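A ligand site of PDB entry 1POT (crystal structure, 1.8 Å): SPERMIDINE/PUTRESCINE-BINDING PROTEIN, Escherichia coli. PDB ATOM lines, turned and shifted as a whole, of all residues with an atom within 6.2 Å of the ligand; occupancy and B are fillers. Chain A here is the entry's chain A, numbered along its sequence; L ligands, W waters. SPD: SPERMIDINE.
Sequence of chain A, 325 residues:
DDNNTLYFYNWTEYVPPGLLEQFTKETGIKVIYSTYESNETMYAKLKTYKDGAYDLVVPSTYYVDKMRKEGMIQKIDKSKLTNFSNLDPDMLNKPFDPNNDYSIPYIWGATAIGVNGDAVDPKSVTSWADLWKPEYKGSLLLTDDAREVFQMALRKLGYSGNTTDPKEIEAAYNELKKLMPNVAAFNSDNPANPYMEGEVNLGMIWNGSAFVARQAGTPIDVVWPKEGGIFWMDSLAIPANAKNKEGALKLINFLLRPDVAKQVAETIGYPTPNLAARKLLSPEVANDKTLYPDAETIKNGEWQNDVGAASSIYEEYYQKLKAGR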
ATOM      1  N   TRP A  11       3.319  -3.541 -22.227  1.00  0.00           N
ATOM      2  CA  TRP A  11       3.957  -4.859 -22.038  1.00  0.00           C
ATOM      3  C   TRP A  11       5.415  -4.651 -22.401  1.00  0.00           C
ATOM      4  O   TRP A  11       5.777  -3.751 -23.143  1.00  0.00           O
ATOM      5  CB  TRP A  11       3.338  -5.963 -22.854  1.00  0.00           C
ATOM      6  CG  TRP A  11       1.883  -6.159 -22.653  1.00  0.00           C
ATOM      7  CD1 TRP A  11       0.903  -5.340 -23.142  1.00  0.00           C
ATOM      8  CD2 TRP A  11       1.215  -7.228 -21.960  1.00  0.00           C
ATOM      9  NE1 TRP A  11      -0.336  -5.831 -22.830  1.00  0.00           N
ATOM     10  CE2 TRP A  11      -0.178  -6.960 -22.042  1.00  0.00           C
ATOM     11  CE3 TRP A  11       1.646  -8.334 -21.253  1.00  0.00           C
ATOM     12  CZ2 TRP A  11      -1.147  -7.788 -21.525  1.00  0.00           C
ATOM     13  CZ3 TRP A  11       0.691  -9.175 -20.708  1.00  0.00           C
ATOM     14  CH2 TRP A  11      -0.664  -8.900 -20.825  1.00  0.00           C
ATOM     15  N   THR A  12       6.226  -5.542 -21.889  1.00  0.00           N
ATOM     16  CA  THR A  12       7.678  -5.529 -22.045  1.00  0.00           C
ATOM     17  C   THR A  12       8.342  -5.613 -23.378  1.00  0.00           C
ATOM     18  O   THR A  12       9.468  -4.934 -23.422  1.00  0.00           O
ATOM     19  CB  THR A  12       8.312  -6.637 -21.085  1.00  0.00           C
ATOM     20  OG1 THR A  12       7.675  -7.874 -21.565  1.00  0.00           O
ATOM     21  CG2 THR A  12       8.017  -6.363 -19.601  1.00  0.00           C
ATOM     22  N   GLU A  13       7.945  -6.296 -24.428  1.00  0.00           N
ATOM     23  CA  GLU A  13       8.926  -6.264 -25.589  1.00  0.00           C
ATOM     24  C   GLU A  13       8.482  -5.544 -26.824  1.00  0.00           C
ATOM     25  O   GLU A  13       9.176  -5.376 -27.834  1.00  0.00           O
ATOM     26  CB  GLU A  13       9.353  -7.693 -25.842  1.00  0.00           C
ATOM     27  CG  GLU A  13       8.350  -8.778 -26.118  1.00  0.00           C
ATOM     28  CD  GLU A  13       8.553 -10.211 -25.837  1.00  0.00           C
ATOM     29  OE1 GLU A  13       9.649 -10.719 -25.758  1.00  0.00           O
ATOM     30  OE2 GLU A  13       7.484 -10.876 -25.731  1.00  0.00           O
ATOM     31  N   TYR A  14       7.294  -4.984 -26.753  1.00  0.00           N
ATOM     32  CA  TYR A  14       6.572  -4.253 -27.745  1.00  0.00           C
ATOM     33  C   TYR A  14       7.154  -2.951 -28.224  1.00  0.00           C
ATOM     34  O   TYR A  14       6.828  -2.726 -29.423  1.00  0.00           O
ATOM     35  CB  TYR A  14       5.143  -3.998 -27.290  1.00  0.00           C
ATOM     36  CG  TYR A  14       4.133  -5.103 -27.337  1.00  0.00           C
ATOM     37  CD1 TYR A  14       4.260  -6.310 -28.009  1.00  0.00           C
ATOM     38  CD2 TYR A  14       2.927  -4.849 -26.617  1.00  0.00           C
ATOM     39  CE1 TYR A  14       3.221  -7.208 -28.007  1.00  0.00           C
ATOM     40  CE2 TYR A  14       1.889  -5.749 -26.651  1.00  0.00           C
ATOM     41  CZ  TYR A  14       2.051  -6.947 -27.323  1.00  0.00           C
ATOM     42  OH  TYR A  14       1.025  -7.849 -27.315  1.00  0.00           O
ATOM     43  N   TYR A  36       5.021  -3.568 -17.920  1.00  0.00           N
ATOM     44  CA  TYR A  36       4.406  -4.556 -17.032  1.00  0.00           C
ATOM     45  C   TYR A  36       4.475  -5.894 -17.761  1.00  0.00           C
ATOM     46  O   TYR A  36       4.643  -5.884 -18.984  1.00  0.00           O
ATOM     47  CB  TYR A  36       2.963  -4.301 -16.632  1.00  0.00           C
ATOM     48  CG  TYR A  36       2.015  -3.998 -17.729  1.00  0.00           C
ATOM     49  CD1 TYR A  36       1.372  -5.045 -18.377  1.00  0.00           C
ATOM     50  CD2 TYR A  36       1.669  -2.686 -18.055  1.00  0.00           C
ATOM     51  CE1 TYR A  36       0.437  -4.796 -19.372  1.00  0.00           C
ATOM     52  CE2 TYR A  36       0.730  -2.441 -19.078  1.00  0.00           C
ATOM     53  CZ  TYR A  36       0.120  -3.489 -19.695  1.00  0.00           C
ATOM     54  OH  TYR A  36      -0.817  -3.321 -20.677  1.00  0.00           O
ATOM     55  N   ASN A  39      -1.552  -8.569 -17.267  1.00  0.00           N
ATOM     56  CA  ASN A  39      -2.756  -7.721 -17.082  1.00  0.00           C
ATOM     57  C   ASN A  39      -3.126  -7.640 -15.598  1.00  0.00           C
ATOM     58  O   ASN A  39      -3.624  -6.614 -15.100  1.00  0.00           O
ATOM     59  CB  ASN A  39      -3.964  -8.244 -17.835  1.00  0.00           C
ATOM     60  CG  ASN A  39      -4.059  -8.083 -19.319  1.00  0.00           C
ATOM     61  OD1 ASN A  39      -4.416  -7.025 -19.862  1.00  0.00           O
ATOM     62  ND2 ASN A  39      -3.832  -9.189 -20.023  1.00  0.00           N
ATOM     63  N   SER A  60      -5.344  -6.504 -22.549  1.00  0.00           N
ATOM     64  CA  SER A  60      -5.779  -7.547 -23.491  1.00  0.00           C
ATOM     65  C   SER A  60      -7.263  -7.244 -23.629  1.00  0.00           C
ATOM     66  O   SER A  60      -7.854  -6.753 -22.658  1.00  0.00           O
ATOM     67  CB  SER A  60      -5.557  -8.945 -22.914  1.00  0.00           C
ATOM     68  OG  SER A  60      -4.133  -9.149 -22.833  1.00  0.00           O
ATOM     69  N   TYR A  62      -9.544  -9.023 -23.263  1.00  0.00           N
ATOM     70  CA  TYR A  62     -10.389  -9.680 -22.221  1.00  0.00           C
ATOM     71  C   TYR A  62     -10.459  -8.900 -20.935  1.00  0.00           C
ATOM     72  O   TYR A  62     -11.213  -9.233 -19.969  1.00  0.00           O
ATOM     73  CB  TYR A  62     -10.053 -11.151 -22.062  1.00  0.00           C
ATOM     74  CG  TYR A  62      -8.673 -11.510 -21.594  1.00  0.00           C
ATOM     75  CD1 TYR A  62      -8.281 -11.524 -20.252  1.00  0.00           C
ATOM     76  CD2 TYR A  62      -7.713 -11.882 -22.576  1.00  0.00           C
ATOM     77  CE1 TYR A  62      -6.985 -11.904 -19.877  1.00  0.00           C
ATOM     78  CE2 TYR A  62      -6.419 -12.214 -22.164  1.00  0.00           C
ATOM     79  CZ  TYR A  62      -6.072 -12.244 -20.842  1.00  0.00           C
ATOM     80  OH  TYR A  62      -4.785 -12.673 -20.580  1.00  0.00           O
ATOM     81  N   THR A 111       0.148 -17.931 -28.345  1.00  0.00           N
ATOM     82  CA  THR A 111       0.937 -18.707 -27.385  1.00  0.00           C
ATOM     83  C   THR A 111       0.813 -20.123 -27.999  1.00  0.00           C
ATOM     84  O   THR A 111      -0.270 -20.549 -28.424  1.00  0.00           O
ATOM     85  CB  THR A 111       0.541 -18.664 -25.890  1.00  0.00           C
ATOM     86  OG1 THR A 111       0.468 -17.308 -25.337  1.00  0.00           O
ATOM     87  CG2 THR A 111       1.599 -19.432 -25.029  1.00  0.00           C
ATOM     88  N   ASP A 145       1.154 -16.369 -16.987  1.00  0.00           N
ATOM     89  CA  ASP A 145      -0.207 -15.844 -17.268  1.00  0.00           C
ATOM     90  C   ASP A 145      -1.281 -16.808 -16.814  1.00  0.00           C
ATOM     91  O   ASP A 145      -1.331 -17.901 -17.407  1.00  0.00           O
ATOM     92  CB  ASP A 145      -0.163 -15.664 -18.783  1.00  0.00           C
ATOM     93  CG  ASP A 145      -1.397 -14.857 -19.189  1.00  0.00           C
ATOM     94  OD1 ASP A 145      -2.449 -15.521 -19.216  1.00  0.00           O
ATOM     95  OD2 ASP A 145      -1.215 -13.648 -19.419  1.00  0.00           O
ATOM     96  N   ARG A 147      -4.575 -16.940 -17.194  1.00  0.00           N
ATOM     97  CA  ARG A 147      -5.483 -17.388 -18.273  1.00  0.00           C
ATOM     98  C   ARG A 147      -4.740 -18.180 -19.340  1.00  0.00           C
ATOM     99  O   ARG A 147      -5.466 -19.013 -19.910  1.00  0.00           O
ATOM    100  CB  ARG A 147      -6.238 -16.234 -18.946  1.00  0.00           C
ATOM    101  CG  ARG A 147      -7.304 -15.608 -18.057  1.00  0.00           C
ATOM    102  CD  ARG A 147      -8.484 -16.474 -17.951  1.00  0.00           C
ATOM    103  NE  ARG A 147      -9.206 -16.675 -19.164  1.00  0.00           N
ATOM    104  CZ  ARG A 147      -9.989 -15.898 -19.858  1.00  0.00           C
ATOM    105  NH1 ARG A 147     -10.318 -14.663 -19.550  1.00  0.00           N
ATOM    106  NH2 ARG A 147     -10.416 -16.399 -21.021  1.00  0.00           N
ATOM    107  N   GLU A 148      -3.484 -17.963 -19.594  1.00  0.00           N
ATOM    108  CA  GLU A 148      -2.848 -18.791 -20.639  1.00  0.00           C
ATOM    109  C   GLU A 148      -2.550 -20.171 -20.083  1.00  0.00           C
ATOM    110  O   GLU A 148      -2.811 -21.134 -20.840  1.00  0.00           O
ATOM    111  CB  GLU A 148      -1.582 -18.153 -21.183  1.00  0.00           C
ATOM    112  CG  GLU A 148      -1.832 -16.910 -22.056  1.00  0.00           C
ATOM    113  CD  GLU A 148      -0.672 -16.272 -22.700  1.00  0.00           C
ATOM    114  OE1 GLU A 148       0.346 -16.979 -22.815  1.00  0.00           O
ATOM    115  OE2 GLU A 148      -0.693 -15.116 -23.137  1.00  0.00           O
ATOM    116  N   SER A 188       7.051 -14.094 -18.082  1.00  0.00           N
ATOM    117  CA  SER A 188       6.145 -13.296 -18.927  1.00  0.00           C
ATOM    118  C   SER A 188       6.872 -12.034 -19.378  1.00  0.00           C
ATOM    119  O   SER A 188       6.296 -11.160 -20.054  1.00  0.00           O
ATOM    120  CB  SER A 188       4.831 -13.024 -18.231  1.00  0.00           C
ATOM    121  OG  SER A 188       3.789 -13.913 -18.527  1.00  0.00           O
ATOM    122  N   ASP A 189       8.152 -11.999 -19.034  1.00  0.00           N
ATOM    123  CA  ASP A 189       9.069 -10.884 -19.351  1.00  0.00           C
ATOM    124  C   ASP A 189       9.495 -10.942 -20.819  1.00  0.00           C
ATOM    125  O   ASP A 189       9.316 -10.060 -21.650  1.00  0.00           O
ATOM    126  CB  ASP A 189      10.248 -10.925 -18.370  1.00  0.00           C
ATOM    127  CG  ASP A 189      11.348  -9.954 -18.770  1.00  0.00           C
ATOM    128  OD1 ASP A 189      11.108  -8.757 -18.992  1.00  0.00           O
ATOM    129  OD2 ASP A 189      12.496 -10.437 -18.892  1.00  0.00           O
ATOM    130  N   ASN A 190      10.107 -12.061 -21.130  1.00  0.00           N
ATOM    131  CA  ASN A 190      10.592 -12.422 -22.477  1.00  0.00           C
ATOM    132  C   ASN A 190      10.887 -13.940 -22.318  1.00  0.00           C
ATOM    133  O   ASN A 190      11.992 -14.289 -21.904  1.00  0.00           O
ATOM    134  CB  ASN A 190      11.770 -11.616 -22.898  1.00  0.00           C
ATOM    135  CG  ASN A 190      12.557 -12.181 -24.045  1.00  0.00           C
ATOM    136  OD1 ASN A 190      12.149 -13.109 -24.749  1.00  0.00           O
ATOM    137  ND2 ASN A 190      13.736 -11.588 -24.235  1.00  0.00           N
ATOM    138  N   PRO A 191       9.872 -14.709 -22.602  1.00  0.00           N
ATOM    139  CA  PRO A 191       9.929 -16.158 -22.484  1.00  0.00           C
ATOM    140  C   PRO A 191      10.947 -16.857 -23.361  1.00  0.00           C
ATOM    141  O   PRO A 191      11.300 -18.026 -23.016  1.00  0.00           O
ATOM    142  CB  PRO A 191       8.487 -16.619 -22.798  1.00  0.00           C
ATOM    143  CG  PRO A 191       8.037 -15.520 -23.733  1.00  0.00           C
ATOM    144  CD  PRO A 191       8.533 -14.244 -23.065  1.00  0.00           C
ATOM    145  N   TRP A 206       5.418 -17.303 -26.737  1.00  0.00           N
ATOM    146  CA  TRP A 206       4.701 -16.223 -27.454  1.00  0.00           C
ATOM    147  C   TRP A 206       5.313 -16.284 -28.848  1.00  0.00           C
ATOM    148  O   TRP A 206       6.537 -16.407 -28.925  1.00  0.00           O
ATOM    149  CB  TRP A 206       4.940 -14.916 -26.716  1.00  0.00           C
ATOM    150  CG  TRP A 206       4.047 -14.724 -25.562  1.00  0.00           C
ATOM    151  CD1 TRP A 206       2.812 -15.281 -25.384  1.00  0.00           C
ATOM    152  CD2 TRP A 206       4.243 -13.882 -24.399  1.00  0.00           C
ATOM    153  NE1 TRP A 206       2.227 -14.877 -24.219  1.00  0.00           N
ATOM    154  CE2 TRP A 206       3.082 -13.999 -23.596  1.00  0.00           C
ATOM    155  CE3 TRP A 206       5.294 -13.083 -24.003  1.00  0.00           C
ATOM    156  CZ2 TRP A 206       2.942 -13.334 -22.381  1.00  0.00           C
ATOM    157  CZ3 TRP A 206       5.137 -12.416 -22.786  1.00  0.00           C
ATOM    158  CH2 TRP A 206       4.003 -12.542 -21.992  1.00  0.00           C
ATOM    159  N   TRP A 232      -4.615 -14.030 -28.743  1.00  0.00           N
ATOM    160  CA  TRP A 232      -4.961 -12.886 -27.860  1.00  0.00           C
ATOM    161  C   TRP A 232      -4.646 -11.612 -28.650  1.00  0.00           C
ATOM    162  O   TRP A 232      -4.045 -11.710 -29.702  1.00  0.00           O
ATOM    163  CB  TRP A 232      -4.168 -12.985 -26.564  1.00  0.00           C
ATOM    164  CG  TRP A 232      -2.706 -13.301 -26.717  1.00  0.00           C
ATOM    165  CD1 TRP A 232      -2.141 -14.534 -26.393  1.00  0.00           C
ATOM    166  CD2 TRP A 232      -1.601 -12.493 -27.157  1.00  0.00           C
ATOM    167  NE1 TRP A 232      -0.821 -14.500 -26.634  1.00  0.00           N
ATOM    168  CE2 TRP A 232      -0.442 -13.290 -27.104  1.00  0.00           C
ATOM    169  CE3 TRP A 232      -1.492 -11.206 -27.613  1.00  0.00           C
ATOM    170  CZ2 TRP A 232       0.826 -12.856 -27.462  1.00  0.00           C
ATOM    171  CZ3 TRP A 232      -0.241 -10.761 -28.014  1.00  0.00           C
ATOM    172  CH2 TRP A 232       0.893 -11.546 -27.901  1.00  0.00           C
ATOM    173  N   MET A 233      -5.069 -10.482 -28.115  1.00  0.00           N
ATOM    174  CA  MET A 233      -4.826  -9.167 -28.734  1.00  0.00           C
ATOM    175  C   MET A 233      -4.675  -8.135 -27.632  1.00  0.00           C
ATOM    176  O   MET A 233      -5.453  -8.205 -26.670  1.00  0.00           O
ATOM    177  CB  MET A 233      -5.959  -8.822 -29.716  1.00  0.00           C
ATOM    178  CG  MET A 233      -5.867  -7.347 -30.012  1.00  0.00           C
ATOM    179  SD  MET A 233      -6.494  -6.949 -31.644  1.00  0.00           S
ATOM    180  CE  MET A 233      -8.217  -7.520 -31.463  1.00  0.00           C
ATOM    181  N   ASP A 234      -3.741  -7.221 -27.824  1.00  0.00           N
ATOM    182  CA  ASP A 234      -3.531  -6.141 -26.841  1.00  0.00           C
ATOM    183  C   ASP A 234      -4.038  -4.857 -27.523  1.00  0.00           C
ATOM    184  O   ASP A 234      -3.727  -4.655 -28.669  1.00  0.00           O
ATOM    185  CB  ASP A 234      -2.144  -6.118 -26.256  1.00  0.00           C
ATOM    186  CG  ASP A 234      -1.734  -7.348 -25.511  1.00  0.00           C
ATOM    187  OD1 ASP A 234      -2.464  -8.018 -24.738  1.00  0.00           O
ATOM    188  OD2 ASP A 234      -0.534  -7.710 -25.653  1.00  0.00           O
ATOM    189  N   TYR A 270       5.845  -9.751 -33.522  1.00  0.00           N
ATOM    190  CA  TYR A 270       4.386  -9.920 -33.245  1.00  0.00           C
ATOM    191  C   TYR A 270       3.646  -9.213 -34.396  1.00  0.00           C
ATOM    192  O   TYR A 270       4.152  -8.177 -34.776  1.00  0.00           O
ATOM    193  CB  TYR A 270       3.896  -9.278 -31.959  1.00  0.00           C
ATOM    194  CG  TYR A 270       4.396  -9.988 -30.712  1.00  0.00           C
ATOM    195  CD1 TYR A 270       3.785 -11.136 -30.269  1.00  0.00           C
ATOM    196  CD2 TYR A 270       5.505  -9.490 -30.013  1.00  0.00           C
ATOM    197  CE1 TYR A 270       4.268 -11.798 -29.151  1.00  0.00           C
ATOM    198  CE2 TYR A 270       5.970 -10.187 -28.916  1.00  0.00           C
ATOM    199  CZ  TYR A 270       5.352 -11.329 -28.487  1.00  0.00           C
ATOM    200  OH  TYR A 270       5.863 -11.951 -27.365  1.00  0.00           O
ATOM    201  N   GLN A 304      -8.592 -15.566 -26.437  1.00  0.00           N
ATOM    202  CA  GLN A 304      -8.838 -15.394 -24.986  1.00  0.00           C
ATOM    203  C   GLN A 304      -9.849 -14.255 -24.872  1.00  0.00           C
ATOM    204  O   GLN A 304      -9.577 -13.141 -25.324  1.00  0.00           O
ATOM    205  CB  GLN A 304      -7.581 -15.090 -24.154  1.00  0.00           C
ATOM    206  CG  GLN A 304      -6.285 -15.818 -24.503  1.00  0.00           C
ATOM    207  CD  GLN A 304      -5.321 -15.841 -23.347  1.00  0.00           C
ATOM    208  OE1 GLN A 304      -4.584 -14.915 -22.997  1.00  0.00           O
ATOM    209  NE2 GLN A 304      -5.337 -16.947 -22.609  1.00  0.00           N
HETATM  210  N1  SPD L   1       5.669  -8.964 -24.067  1.00  0.00           N
HETATM  211  C2  SPD L   1       4.786  -8.547 -25.214  1.00  0.00           C
HETATM  212  C3  SPD L   1       3.836  -9.753 -25.514  1.00  0.00           C
HETATM  213  C4  SPD L   1       2.717  -9.644 -24.494  1.00  0.00           C
HETATM  214  C5  SPD L   1       1.488 -10.392 -24.864  1.00  0.00           C
HETATM  215  N6  SPD L   1       0.428  -9.949 -23.996  1.00  0.00           N
HETATM  216  C7  SPD L   1      -0.887 -10.415 -23.973  1.00  0.00           C
HETATM  217  C8  SPD L   1      -0.982 -11.730 -23.254  1.00  0.00           C
HETATM  218  C9  SPD L   1      -2.337 -12.298 -23.353  1.00  0.00           C
HETATM  219  N10 SPD L   1      -2.599 -13.283 -22.228  1.00  0.00           N
HETATM  220  O   HOH W   1       4.973  -9.293 -21.464  1.00  0.00           O
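Water W1 lies within hydrogen-bond range of O of Ser 188 (2.7 Å), N1 of the ligand (2.7 Å) and OG1 of Thr 12 (3.1 Å).
The side-chain amide nitrogen (NE2) of Gln 304 lies within hydrogen-bond range of the backbone carbonyl oxygen (O) of Arg 147 (3.4 Å).
The backbone NH (N) of Glu 148 sits at hydrogen-bond distance from the side-chain carboxylate (OD1) of Asp 145 (2.7 Å).
OG1 of Thr 111 sits at hydrogen-bond distance from OE1 of Glu 148, 2.5 Å away.
The indole nitrogen of Trp 11 lies close to the side-chain carboxylate of Asp 234, at 3.4 Å.
The backbone NH of Arg 147 lies within hydrogen-bond range of the side-chain carboxylate of Asp 145, at 3.3 Å.
N of Thr 12 is in hydrogen-bond range of O of Tyr 36, at 3.3 Å.
The side-chain hydroxyl of Ser 60 lies within hydrogen-bond range of the side-chain amide nitrogen of Asn 39 (2.8 Å).
The indole nitrogen (NE1) of Trp 206 sits close to the side-chain hydroxyl (OG1) of Thr 111, at 3.2 Å.
Residues that only touch the ligand: Trp 232 (3.3 Å), Trp 11 (3.4 Å), Tyr 14 (3.5 Å), Tyr 270 (3.5 Å), Ser 60 (3.7 Å) and Trp 206 (3.7 Å).
The side-chain amide oxygen (OE1) of Gln 304 lies within hydrogen-bond range of a nitrogen (N10) of the ligand, 2.7 Å away.
The side-chain carboxylate (OE2) of Glu 148 is in salt-bridge range of a nitrogen (N10) of the ligand (2.8 Å).
N10 of the ligand sits at hydrogen-bond distance from OH of Tyr 62 (2.8 Å).
A nitrogen (N6) of the ligand is in salt-bridge range of the side-chain carboxylate of Asp 234.
OE2 of Glu 13 lies within salt-bridge range of N1 of the ligand, at 3.1 Å.
The side-chain carboxylate of Asp 145 is in salt-bridge range of a nitrogen (N10) of the ligand, 3.2 Å away.
A nitrogen (N1) of the ligand lies within hydrogen-bond range of the side-chain hydroxyl (OG1) of Thr 12 (3.4 Å).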
